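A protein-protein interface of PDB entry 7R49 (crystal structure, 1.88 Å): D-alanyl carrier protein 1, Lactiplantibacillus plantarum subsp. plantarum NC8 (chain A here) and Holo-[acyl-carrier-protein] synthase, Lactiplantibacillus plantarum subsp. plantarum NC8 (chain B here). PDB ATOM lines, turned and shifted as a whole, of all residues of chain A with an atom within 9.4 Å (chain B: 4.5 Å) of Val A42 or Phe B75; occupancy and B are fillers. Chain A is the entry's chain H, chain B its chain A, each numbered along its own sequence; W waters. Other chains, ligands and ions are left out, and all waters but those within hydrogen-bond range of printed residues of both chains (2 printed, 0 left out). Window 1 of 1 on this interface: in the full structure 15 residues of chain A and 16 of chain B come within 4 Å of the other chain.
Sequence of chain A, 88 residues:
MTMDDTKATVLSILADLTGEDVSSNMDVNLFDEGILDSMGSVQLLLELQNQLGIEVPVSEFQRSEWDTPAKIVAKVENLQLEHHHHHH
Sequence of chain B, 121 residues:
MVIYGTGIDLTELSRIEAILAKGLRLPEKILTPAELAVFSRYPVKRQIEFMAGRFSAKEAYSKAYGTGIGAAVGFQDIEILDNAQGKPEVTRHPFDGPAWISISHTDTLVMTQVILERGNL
NZ of Lys B29 is in salt-bridge range of OE1 of Glu A55 (3.7 Å). NZ of Lys B29 is in hydrogen-bond range of O of Val A56 (3.0 Å).
NE2 of Gln B76 is in hydrogen-bond range of O of Lys B29, 3.0 Å away. N of Gly B74 lies within hydrogen-bond range of OD2 of Asp B77, 2.8 Å away. O of Phe B75 sits at hydrogen-bond distance from NZ of Lys B58 (3.0 Å). The backbone NH (N) of Glu A55 is in hydrogen-bond range of the side-chain amide oxygen (OE1) of Gln A49. The side-chain hydroxyl of Ser A41 lies within hydrogen-bond range of the backbone carbonyl oxygen of Ser A38 (3.2 Å). The backbone NH of Met A39 sits at hydrogen-bond distance from the side-chain carboxylate of Asp A37 (3.0 Å).
Glu B59 touches Ser A38. Met A39 touches Phe B55. CG1 of Val A42 touches CD1 of Leu B26, 3.7 Å away. Val A42 touches Phe B55 (CG2 to CE1, 3.9998 Å). CG2 of Val A42 touches CZ of Phe B75 (3.6 Å). Leu A45 touches Lys B29. Leu B26 touches Leu A46 (CA to CD1, 3.9 Å). CD2 of Leu A46 touches CB of Lys B29, at 3.97 Å. Val A58 touches Ile B69 (CG1 to CG2, 3.6 Å). CG1 of Val A58 touches CA of Gly B74, at 3.9 Å.
Leu A17 touches none of the printed residues of chain B. Of the printed residues of chain B, Met A39 touches Phe B55. Printed residues of chain B within 4 Å of Val A42: Leu B26, Phe B55 and Phe B75. Printed residues of chain A within 4 Å of Leu B26: Val A42 (3.7 Å) and Leu A46 (3.9 Å). Of the printed residues of chain A, Lys B29 touches Leu A45, Leu A46, Glu A55 and Val A56. Of the printed residues of chain A, Ile B69 touches Val A58 (3.6 Å). Phe B75 touches one residue of chain A. No residue of chain A comes within 4 Å of Gln B76. The nearest printed residue of chain A that does not touch Leu B26 is Gln A43 (6.0 Å).
Of the 24 printed residues of chain A, 8 touch a printed residue of chain B. Printed residues of chain B that touch a printed residue of chain A: Leu B26, Lys B29, Phe B55, Glu B59, Ile B69, Gly B74 and Phe B75. Along chain B the printed residues that touch a printed residue of chain A span positions 26 to 75. Among the printed residues, Asp or Glu carboxylates within 4 Å of a Lys or Arg side-chain nitrogen of the other chain: Glu A55 with Lys B29 (3.7 Å).
Water W2 bridges the side-chain carboxylate of Glu B59 (2.7 Å) and the side-chain hydroxyl of Ser A38 (2.9 Å). Water W1 lies within hydrogen-bond range of NZ of Lys B29 (2.9 Å), O of Leu A45 (3.3 Å) and OE1 of Glu A55 (3.5 Å).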
ATOM      1  N   ILE A  13      23.501 -11.138  16.097  1.00  0.00           N
ATOM      2  CA  ILE A  13      23.262  -9.900  15.347  1.00  0.00           C
ATOM      3  C   ILE A  13      24.070  -9.880  14.048  1.00  0.00           C
ATOM      4  O   ILE A  13      23.535  -9.626  12.962  1.00  0.00           O
ATOM      5  CB  ILE A  13      23.583  -8.674  16.223  1.00  0.00           C
ATOM      6  CG1 ILE A  13      22.541  -8.512  17.329  1.00  0.00           C
ATOM      7  CG2 ILE A  13      23.689  -7.406  15.365  1.00  0.00           C
ATOM      8  CD1 ILE A  13      23.008  -7.603  18.421  1.00  0.00           C
ATOM      9  N   LEU A  17      22.839  -9.742  10.095  1.00  0.00           N
ATOM     10  CA  LEU A  17      23.188  -8.613   9.236  1.00  0.00           C
ATOM     11  C   LEU A  17      23.921  -9.078   7.983  1.00  0.00           C
ATOM     12  O   LEU A  17      23.664  -8.583   6.880  1.00  0.00           O
ATOM     13  CB  LEU A  17      24.041  -7.611  10.026  1.00  0.00           C
ATOM     14  CG  LEU A  17      23.318  -6.831  11.140  1.00  0.00           C
ATOM     15  CD1 LEU A  17      24.238  -5.859  11.875  1.00  0.00           C
ATOM     16  CD2 LEU A  17      22.135  -6.064  10.543  1.00  0.00           C
ATOM     17  N   PHE A  31      33.949  -5.977   6.109  1.00  0.00           N
ATOM     18  CA  PHE A  31      33.756  -4.909   5.135  1.00  0.00           C
ATOM     19  C   PHE A  31      34.461  -5.217   3.827  1.00  0.00           C
ATOM     20  O   PHE A  31      33.899  -5.005   2.747  1.00  0.00           O
ATOM     21  CB  PHE A  31      34.254  -3.597   5.721  1.00  0.00           C
ATOM     22  CG  PHE A  31      33.431  -3.126   6.870  1.00  0.00           C
ATOM     23  CD1 PHE A  31      32.243  -2.462   6.653  1.00  0.00           C
ATOM     24  CD2 PHE A  31      33.809  -3.423   8.173  1.00  0.00           C
ATOM     25  CE1 PHE A  31      31.470  -2.047   7.722  1.00  0.00           C
ATOM     26  CE2 PHE A  31      33.043  -3.009   9.252  1.00  0.00           C
ATOM     27  CZ  PHE A  31      31.880  -2.323   9.031  1.00  0.00           C
ATOM     28  N   LEU A  36      29.308  -6.970   5.242  1.00  0.00           N
ATOM     29  CA  LEU A  36      28.788  -5.868   6.037  1.00  0.00           C
ATOM     30  C   LEU A  36      29.185  -4.570   5.362  1.00  0.00           C
ATOM     31  O   LEU A  36      30.292  -4.464   4.834  1.00  0.00           O
ATOM     32  CB  LEU A  36      29.317  -5.909   7.484  1.00  0.00           C
ATOM     33  CG  LEU A  36      28.606  -4.962   8.448  1.00  0.00           C
ATOM     34  CD1 LEU A  36      27.223  -5.471   8.736  1.00  0.00           C
ATOM     35  CD2 LEU A  36      29.384  -4.902   9.754  1.00  0.00           C
ATOM     36  N   ASP A  37      28.281  -3.600   5.353  1.00  0.00           N
ATOM     37  CA  ASP A  37      28.608  -2.349   4.747  1.00  0.00           C
ATOM     38  C   ASP A  37      28.232  -1.236   5.740  1.00  0.00           C
ATOM     39  O   ASP A  37      27.984  -1.515   6.901  1.00  0.00           O
ATOM     40  CB  ASP A  37      27.859  -2.197   3.418  1.00  0.00           C
ATOM     41  CG  ASP A  37      26.346  -2.059   3.579  1.00  0.00           C
ATOM     42  OD1 ASP A  37      25.775  -2.020   4.703  1.00  0.00           O
ATOM     43  OD2 ASP A  37      25.690  -1.940   2.533  1.00  0.00           O
ATOM     44  N   SER A  38      28.127   0.003   5.260  1.00  0.00           N
ATOM     45  CA  SER A  38      27.903   1.136   6.129  1.00  0.00           C
ATOM     46  C   SER A  38      26.807   1.150   6.805  1.00  0.00           C
ATOM     47  O   SER A  38      26.521   1.623   7.830  1.00  0.00           O
ATOM     48  CB  SER A  38      28.262   2.457   5.424  1.00  0.00           C
ATOM     49  OG  SER A  38      28.948   2.471   4.158  1.00  0.00           O
ATOM     50  N   MET A  39      25.796   0.702   6.029  1.00  0.00           N
ATOM     51  CA  MET A  39      24.428   0.759   6.536  1.00  0.00           C
ATOM     52  C   MET A  39      24.268  -0.313   7.603  1.00  0.00           C
ATOM     53  O   MET A  39      23.703  -0.067   8.675  1.00  0.00           O
ATOM     54  CB  MET A  39      23.351   0.590   5.474  1.00  0.00           C
ATOM     55  CG  MET A  39      22.059   1.140   6.021  1.00  0.00           C
ATOM     56  SD  MET A  39      20.645   0.854   4.946  1.00  0.00           S
ATOM     57  CE  MET A  39      21.207   1.826   3.521  1.00  0.00           C
ATOM     58  N   GLY A  40      24.820  -1.489   7.301  1.00  0.00           N
ATOM     59  CA  GLY A  40      24.814  -2.578   8.258  1.00  0.00           C
ATOM     60  C   GLY A  40      25.510  -2.227   9.558  1.00  0.00           C
ATOM     61  O   GLY A  40      25.092  -2.668  10.630  1.00  0.00           O
ATOM     62  N   SER A  41      26.587  -1.447   9.472  1.00  0.00           N
ATOM     63  CA  SER A  41      27.328  -1.039  10.655  1.00  0.00           C
ATOM     64  C   SER A  41      26.498  -0.090  11.522  1.00  0.00           C
ATOM     65  O   SER A  41      26.583  -0.152  12.754  1.00  0.00           O
ATOM     66  CB  SER A  41      28.685  -0.446  10.223  1.00  0.00           C
ATOM     67  OG  SER A  41      28.680   0.985  10.089  1.00  0.00           O
ATOM     68  N   VAL A  42      25.655   0.751  10.915  1.00  0.00           N
ATOM     69  CA  VAL A  42      24.697   1.523  11.706  1.00  0.00           C
ATOM     70  C   VAL A  42      23.641   0.606  12.317  1.00  0.00           C
ATOM     71  O   VAL A  42      23.275   0.753  13.490  1.00  0.00           O
ATOM     72  CB  VAL A  42      24.033   2.623  10.861  1.00  0.00           C
ATOM     73  CG1 VAL A  42      22.889   3.274  11.664  1.00  0.00           C
ATOM     74  CG2 VAL A  42      25.060   3.665  10.412  1.00  0.00           C
ATOM     75  N   GLN A  43      23.110  -0.340  11.530  1.00  0.00           N
ATOM     76  CA  GLN A  43      22.112  -1.251  12.092  1.00  0.00           C
ATOM     77  C   GLN A  43      22.708  -2.056  13.233  1.00  0.00           C
ATOM     78  O   GLN A  43      22.022  -2.340  14.225  1.00  0.00           O
ATOM     79  CB  GLN A  43      21.528  -2.197  11.037  1.00  0.00           C
ATOM     80  CG  GLN A  43      20.135  -2.674  11.450  1.00  0.00           C
ATOM     81  CD  GLN A  43      19.492  -3.664  10.489  1.00  0.00           C
ATOM     82  OE1 GLN A  43      19.631  -3.556   9.256  1.00  0.00           O
ATOM     83  NE2 GLN A  43      18.787  -4.650  11.060  1.00  0.00           N
ATOM     84  N   LEU A  44      23.990  -2.410  13.117  1.00  0.00           N
ATOM     85  CA  LEU A  44      24.701  -3.052  14.214  1.00  0.00           C
ATOM     86  C   LEU A  44      24.623  -2.214  15.487  1.00  0.00           C
ATOM     87  O   LEU A  44      24.343  -2.739  16.572  1.00  0.00           O
ATOM     88  CB  LEU A  44      26.165  -3.287  13.823  1.00  0.00           C
ATOM     89  CG  LEU A  44      27.061  -3.746  14.975  1.00  0.00           C
ATOM     90  CD1 LEU A  44      26.678  -5.162  15.346  1.00  0.00           C
ATOM     91  CD2 LEU A  44      28.583  -3.635  14.676  1.00  0.00           C
ATOM     92  N   LEU A  45      24.874  -0.904  15.385  1.00  0.00           N
ATOM     93  CA  LEU A  45      24.788  -0.092  16.599  1.00  0.00           C
ATOM     94  C   LEU A  45      23.359  -0.068  17.151  1.00  0.00           C
ATOM     95  O   LEU A  45      23.151  -0.171  18.365  1.00  0.00           O
ATOM     96  CB  LEU A  45      25.298   1.327  16.360  1.00  0.00           C
ATOM     97  CG  LEU A  45      26.733   1.528  15.829  1.00  0.00           C
ATOM     98  CD1 LEU A  45      27.035   3.017  15.764  1.00  0.00           C
ATOM     99  CD2 LEU A  45      27.753   0.818  16.678  1.00  0.00           C
ATOM    100  N   LEU A  46      22.366   0.053  16.277  1.00  0.00           N
ATOM    101  CA  LEU A  46      20.983   0.101  16.736  1.00  0.00           C
ATOM    102  C   LEU A  46      20.581  -1.201  17.417  1.00  0.00           C
ATOM    103  O   LEU A  46      19.814  -1.194  18.388  1.00  0.00           O
ATOM    104  CB  LEU A  46      20.042   0.395  15.565  1.00  0.00           C
ATOM    105  CG  LEU A  46      20.231   1.716  14.809  1.00  0.00           C
ATOM    106  CD1 LEU A  46      19.326   1.722  13.574  1.00  0.00           C
ATOM    107  CD2 LEU A  46      19.969   2.930  15.700  1.00  0.00           C
ATOM    108  N   GLU A  47      21.062  -2.329  16.899  1.00  0.00           N
ATOM    109  CA  GLU A  47      20.718  -3.626  17.464  1.00  0.00           C
ATOM    110  C   GLU A  47      21.389  -3.840  18.814  1.00  0.00           C
ATOM    111  O   GLU A  47      20.782  -4.391  19.737  1.00  0.00           O
ATOM    112  CB  GLU A  47      21.124  -4.719  16.479  1.00  0.00           C
ATOM    113  CG  GLU A  47      20.290  -4.715  15.196  1.00  0.00           C
ATOM    114  CD  GLU A  47      18.885  -5.295  15.360  1.00  0.00           C
ATOM    115  OE1 GLU A  47      18.434  -5.558  16.515  1.00  0.00           O
ATOM    116  OE2 GLU A  47      18.224  -5.489  14.302  1.00  0.00           O
ATOM    117  N   LEU A  48      22.640  -3.395  18.946  1.00  0.00           N
ATOM    118  CA  LEU A  48      23.355  -3.524  20.208  1.00  0.00           C
ATOM    119  C   LEU A  48      22.627  -2.772  21.314  1.00  0.00           C
ATOM    120  O   LEU A  48      22.415  -3.302  22.415  1.00  0.00           O
ATOM    121  CB  LEU A  48      24.779  -2.994  20.041  1.00  0.00           C
ATOM    122  CG  LEU A  48      25.731  -3.833  19.184  1.00  0.00           C
ATOM    123  CD1 LEU A  48      27.052  -3.100  19.114  1.00  0.00           C
ATOM    124  CD2 LEU A  48      25.898  -5.275  19.746  1.00  0.00           C
ATOM    125  N   GLN A  49      22.228  -1.532  21.031  1.00  0.00           N
ATOM    126  CA  GLN A  49      21.419  -0.780  21.982  1.00  0.00           C
ATOM    127  C   GLN A  49      20.068  -1.458  22.206  1.00  0.00           C
ATOM    128  O   GLN A  49      19.683  -1.720  23.349  1.00  0.00           O
ATOM    129  CB  GLN A  49      21.264   0.669  21.494  1.00  0.00           C
ATOM    130  CG  GLN A  49      20.164   1.505  22.166  1.00  0.00           C
ATOM    131  CD  GLN A  49      20.382   1.741  23.662  1.00  0.00           C
ATOM    132  OE1 GLN A  49      21.401   1.337  24.238  1.00  0.00           O
ATOM    133  NE2 GLN A  49      19.409   2.394  24.299  1.00  0.00           N
ATOM    134  N   ASN A  50      19.345  -1.805  21.126  1.00  0.00           N
ATOM    135  CA  ASN A  50      18.013  -2.377  21.339  1.00  0.00           C
ATOM    136  C   ASN A  50      18.079  -3.701  22.091  1.00  0.00           C
ATOM    137  O   ASN A  50      17.270  -3.948  22.990  1.00  0.00           O
ATOM    138  CB  ASN A  50      17.255  -2.600  20.027  1.00  0.00           C
ATOM    139  CG  ASN A  50      15.772  -2.937  20.281  1.00  0.00           C
ATOM    140  OD1 ASN A  50      15.081  -2.197  20.973  1.00  0.00           O
ATOM    141  ND2 ASN A  50      15.315  -4.083  19.792  1.00  0.00           N
ATOM    142  N   GLU A  55      24.647   1.258  24.383  1.00  0.00           N
ATOM    143  CA  GLU A  55      24.722   2.294  23.373  1.00  0.00           C
ATOM    144  C   GLU A  55      26.167   2.559  23.019  1.00  0.00           C
ATOM    145  O   GLU A  55      27.003   2.806  23.891  1.00  0.00           O
ATOM    146  CB  GLU A  55      24.055   3.587  23.825  1.00  0.00           C
ATOM    147  CG  GLU A  55      24.078   4.604  22.693  1.00  0.00           C
ATOM    148  CD  GLU A  55      22.799   5.379  22.571  1.00  0.00           C
ATOM    149  OE1 GLU A  55      22.394   5.657  21.417  1.00  0.00           O
ATOM    150  OE2 GLU A  55      22.181   5.681  23.619  1.00  0.00           O
ATOM    151  N   VAL A  56      26.456   2.505  21.730  1.00  0.00           N
ATOM    152  CA  VAL A  56      27.783   2.817  21.240  1.00  0.00           C
ATOM    153  C   VAL A  56      27.652   4.144  20.506  1.00  0.00           C
ATOM    154  O   VAL A  56      27.066   4.188  19.416  1.00  0.00           O
ATOM    155  CB  VAL A  56      28.312   1.687  20.344  1.00  0.00           C
ATOM    156  CG1 VAL A  56      29.751   1.959  19.931  1.00  0.00           C
ATOM    157  CG2 VAL A  56      28.162   0.342  21.071  1.00  0.00           C
ATOM    158  N   PRO A  57      28.137   5.246  21.062  1.00  0.00           N
ATOM    159  CA  PRO A  57      28.160   6.482  20.283  1.00  0.00           C
ATOM    160  C   PRO A  57      29.115   6.373  19.105  1.00  0.00           C
ATOM    161  O   PRO A  57      30.131   5.673  19.155  1.00  0.00           O
ATOM    162  CB  PRO A  57      28.599   7.532  21.306  1.00  0.00           C
ATOM    163  CG  PRO A  57      29.377   6.738  22.370  1.00  0.00           C
ATOM    164  CD  PRO A  57      29.236   5.256  22.040  1.00  0.00           C
ATOM    165  N   VAL A  58      28.750   7.058  18.018  1.00  0.00           N
ATOM    166  CA  VAL A  58      29.526   6.968  16.783  1.00  0.00           C
ATOM    167  C   VAL A  58      30.950   7.460  16.997  1.00  0.00           C
ATOM    168  O   VAL A  58      31.875   7.011  16.309  1.00  0.00           O
ATOM    169  CB  VAL A  58      28.802   7.727  15.649  1.00  0.00           C
ATOM    170  CG1 VAL A  58      29.684   7.842  14.403  1.00  0.00           C
ATOM    171  CG2 VAL A  58      27.491   7.013  15.305  1.00  0.00           C
ATOM    172  N   SER A  59      31.170   8.338  17.983  1.00  0.00           N
ATOM    173  CA  SER A  59      32.540   8.756  18.286  1.00  0.00           C
ATOM    174  C   SER A  59      33.423   7.583  18.725  1.00  0.00           C
ATOM    175  O   SER A  59      34.648   7.651  18.562  1.00  0.00           O
ATOM    176  CB  SER A  59      32.555   9.857  19.354  1.00  0.00           C
ATOM    177  OG  SER A  59      31.869   9.463  20.526  1.00  0.00           O
ATOM    178  N   PHE A  61      33.226   4.551  17.390  1.00  0.00           N
ATOM    179  CA  PHE A  61      33.146   3.567  16.324  1.00  0.00           C
ATOM    180  C   PHE A  61      34.115   3.948  15.217  1.00  0.00           C
ATOM    181  O   PHE A  61      33.980   5.010  14.605  1.00  0.00           O
ATOM    182  CB  PHE A  61      31.710   3.438  15.809  1.00  0.00           C
ATOM    183  CG  PHE A  61      31.519   2.309  14.842  1.00  0.00           C
ATOM    184  CD1 PHE A  61      31.938   2.440  13.508  1.00  0.00           C
ATOM    185  CD2 PHE A  61      31.050   1.079  15.284  1.00  0.00           C
ATOM    186  CE1 PHE A  61      31.798   1.388  12.601  1.00  0.00           C
ATOM    187  CE2 PHE A  61      30.920   0.015  14.399  1.00  0.00           C
ATOM    188  CZ  PHE A  61      31.299   0.172  13.044  1.00  0.00           C
ATOM    189  N   LEU B  26      16.598   4.559  13.830  1.00  0.00           N
ATOM    190  CA  LEU B  26      17.506   5.125  12.834  1.00  0.00           C
ATOM    191  C   LEU B  26      17.394   6.642  12.697  1.00  0.00           C
ATOM    192  O   LEU B  26      18.438   7.301  12.524  1.00  0.00           O
ATOM    193  CB  LEU B  26      17.250   4.447  11.478  1.00  0.00           C
ATOM    194  CG  LEU B  26      18.115   4.945  10.338  1.00  0.00           C
ATOM    195  CD1 LEU B  26      19.522   4.424  10.572  1.00  0.00           C
ATOM    196  CD2 LEU B  26      17.562   4.470   8.992  1.00  0.00           C
ATOM    197  N   LYS B  29      19.336   8.386  15.369  1.00  0.00           N
ATOM    198  CA  LYS B  29      20.777   8.159  15.255  1.00  0.00           C
ATOM    199  C   LYS B  29      21.412   9.026  14.167  1.00  0.00           C
ATOM    200  O   LYS B  29      22.513   9.545  14.358  1.00  0.00           O
ATOM    201  CB  LYS B  29      21.058   6.673  14.969  1.00  0.00           C
ATOM    202  CG  LYS B  29      22.491   6.254  15.205  1.00  0.00           C
ATOM    203  CD  LYS B  29      22.780   6.047  16.691  1.00  0.00           C
ATOM    204  CE  LYS B  29      23.949   5.103  16.951  1.00  0.00           C
ATOM    205  NZ  LYS B  29      24.477   5.263  18.355  1.00  0.00           N
ATOM    206  N   ILE B  30      20.761   9.150  13.003  1.00  0.00           N
ATOM    207  CA  ILE B  30      21.374   9.746  11.816  1.00  0.00           C
ATOM    208  C   ILE B  30      21.116  11.242  11.685  1.00  0.00           C
ATOM    209  O   ILE B  30      21.947  11.957  11.118  1.00  0.00           O
ATOM    210  CB  ILE B  30      20.883   9.047  10.526  1.00  0.00           C
ATOM    211  CG1 ILE B  30      21.140   7.550  10.579  1.00  0.00           C
ATOM    212  CG2 ILE B  30      21.556   9.643   9.304  1.00  0.00           C
ATOM    213  CD1 ILE B  30      22.559   7.236  10.727  1.00  0.00           C
ATOM    214  N   PHE B  55      21.193   9.869   5.203  1.00  0.00           N
ATOM    215  CA  PHE B  55      22.186   8.838   5.423  1.00  0.00           C
ATOM    216  C   PHE B  55      23.213   8.857   4.303  1.00  0.00           C
ATOM    217  O   PHE B  55      24.427   8.860   4.540  1.00  0.00           O
ATOM    218  CB  PHE B  55      21.509   7.473   5.497  1.00  0.00           C
ATOM    219  CG  PHE B  55      22.485   6.362   5.562  1.00  0.00           C
ATOM    220  CD1 PHE B  55      23.191   6.113   6.731  1.00  0.00           C
ATOM    221  CD2 PHE B  55      22.758   5.606   4.436  1.00  0.00           C
ATOM    222  CE1 PHE B  55      24.134   5.082   6.788  1.00  0.00           C
ATOM    223  CE2 PHE B  55      23.705   4.579   4.486  1.00  0.00           C
ATOM    224  CZ  PHE B  55      24.385   4.323   5.657  1.00  0.00           C
ATOM    225  N   LYS B  58      25.533  11.972   4.225  1.00  0.00           N
ATOM    226  CA  LYS B  58      26.534  12.039   5.282  1.00  0.00           C
ATOM    227  C   LYS B  58      27.600  10.966   5.107  1.00  0.00           C
ATOM    228  O   LYS B  58      28.759  11.207   5.461  1.00  0.00           O
ATOM    229  CB  LYS B  58      25.880  11.917   6.644  1.00  0.00           C
ATOM    230  CG  LYS B  58      24.945  13.071   6.911  1.00  0.00           C
ATOM    231  CD  LYS B  58      24.268  12.943   8.268  1.00  0.00           C
ATOM    232  CE  LYS B  58      23.171  14.014   8.399  1.00  0.00           C
ATOM    233  NZ  LYS B  58      22.778  14.282   9.802  1.00  0.00           N
ATOM    234  N   GLU B  59      27.235   9.785   4.586  1.00  0.00           N
ATOM    235  CA  GLU B  59      28.250   8.828   4.156  1.00  0.00           C
ATOM    236  C   GLU B  59      29.153   9.427   3.080  1.00  0.00           C
ATOM    237  O   GLU B  59      30.380   9.340   3.181  1.00  0.00           O
ATOM    238  CB  GLU B  59      27.607   7.535   3.632  1.00  0.00           C
ATOM    239  CG  GLU B  59      26.956   6.638   4.685  1.00  0.00           C
ATOM    240  CD  GLU B  59      27.952   6.118   5.726  1.00  0.00           C
ATOM    241  OE1 GLU B  59      29.163   6.001   5.430  1.00  0.00           O
ATOM    242  OE2 GLU B  59      27.517   5.809   6.847  1.00  0.00           O
ATOM    243  N   ILE B  69      32.437   7.502   8.363  1.00  0.00           N
ATOM    244  CA  ILE B  69      31.750   7.882   9.587  1.00  0.00           C
ATOM    245  C   ILE B  69      32.430   7.190  10.757  1.00  0.00           C
ATOM    246  O   ILE B  69      32.736   5.987  10.711  1.00  0.00           O
ATOM    247  CB  ILE B  69      30.254   7.536   9.505  1.00  0.00           C
ATOM    248  CG1 ILE B  69      29.573   8.362   8.411  1.00  0.00           C
ATOM    249  CG2 ILE B  69      29.554   7.805  10.835  1.00  0.00           C
ATOM    250  CD1 ILE B  69      29.443   9.889   8.751  1.00  0.00           C
ATOM    251  N   GLY B  74      30.966  12.194  12.706  1.00  0.00           N
ATOM    252  CA  GLY B  74      29.774  11.411  12.923  1.00  0.00           C
ATOM    253  C   GLY B  74      28.584  12.029  12.214  1.00  0.00           C
ATOM    254  O   GLY B  74      28.642  13.125  11.668  1.00  0.00           O
ATOM    255  N   PHE B  75      27.470  11.304  12.260  1.00  0.00           N
ATOM    256  CA  PHE B  75      26.257  11.800  11.621  1.00  0.00           C
ATOM    257  C   PHE B  75      25.787  13.117  12.217  1.00  0.00           C
ATOM    258  O   PHE B  75      25.244  13.963  11.494  1.00  0.00           O
ATOM    259  CB  PHE B  75      25.166  10.759  11.746  1.00  0.00           C
ATOM    260  CG  PHE B  75      25.509   9.470  11.062  1.00  0.00           C
ATOM    261  CD1 PHE B  75      25.594   9.417   9.676  1.00  0.00           C
ATOM    262  CD2 PHE B  75      25.759   8.328  11.801  1.00  0.00           C
ATOM    263  CE1 PHE B  75      25.904   8.231   9.033  1.00  0.00           C
ATOM    264  CE2 PHE B  75      26.073   7.127  11.167  1.00  0.00           C
ATOM    265  CZ  PHE B  75      26.144   7.080   9.791  1.00  0.00           C
ATOM    266  N   GLN B  76      25.957  13.289  13.529  1.00  0.00           N
ATOM    267  CA  GLN B  76      25.507  14.478  14.240  1.00  0.00           C
ATOM    268  C   GLN B  76      26.395  15.691  13.995  1.00  0.00           C
ATOM    269  O   GLN B  76      26.000  16.795  14.378  1.00  0.00           O
ATOM    270  CB  GLN B  76      25.434  14.190  15.746  1.00  0.00           C
ATOM    271  CG  GLN B  76      24.410  13.121  16.161  1.00  0.00           C
ATOM    272  CD  GLN B  76      22.990  13.455  15.725  1.00  0.00           C
ATOM    273  OE1 GLN B  76      22.548  14.593  15.841  1.00  0.00           O
ATOM    274  NE2 GLN B  76      22.277  12.459  15.196  1.00  0.00           N
ATOM    275  N   ASP B  77      27.564  15.518  13.364  1.00  0.00           N
ATOM    276  CA  ASP B  77      28.439  16.619  12.982  1.00  0.00           C
ATOM    277  C   ASP B  77      28.073  17.234  11.641  1.00  0.00           C
ATOM    278  O   ASP B  77      28.626  18.271  11.290  1.00  0.00           O
ATOM    279  CB  ASP B  77      29.897  16.156  12.918  1.00  0.00           C
ATOM    280  CG  ASP B  77      30.377  15.549  14.217  1.00  0.00           C
ATOM    281  OD1 ASP B  77      29.921  16.021  15.273  1.00  0.00           O
ATOM    282  OD2 ASP B  77      31.181  14.580  14.183  1.00  0.00           O
ATOM    283  N   ILE B  78      27.180  16.616  10.876  1.00  0.00           N
ATOM    284  CA  ILE B  78      26.820  17.092   9.547  1.00  0.00           C
ATOM    285  C   ILE B  78      25.329  17.408   9.542  1.00  0.00           C
ATOM    286  O   ILE B  78      24.513  16.588   9.972  1.00  0.00           O
ATOM    287  CB  ILE B  78      27.174  16.054   8.457  1.00  0.00           C
ATOM    288  CG1 ILE B  78      28.637  15.623   8.558  1.00  0.00           C
ATOM    289  CG2 ILE B  78      26.833  16.570   7.053  1.00  0.00           C
ATOM    290  CD1 ILE B  78      28.902  14.224   7.970  1.00  0.00           C
HETATM  291  O   HOH W   1      22.937   2.979  19.283  1.00  0.00           O
HETATM  292  O   HOH W   2      30.224   4.903   3.264  1.00  0.00           O
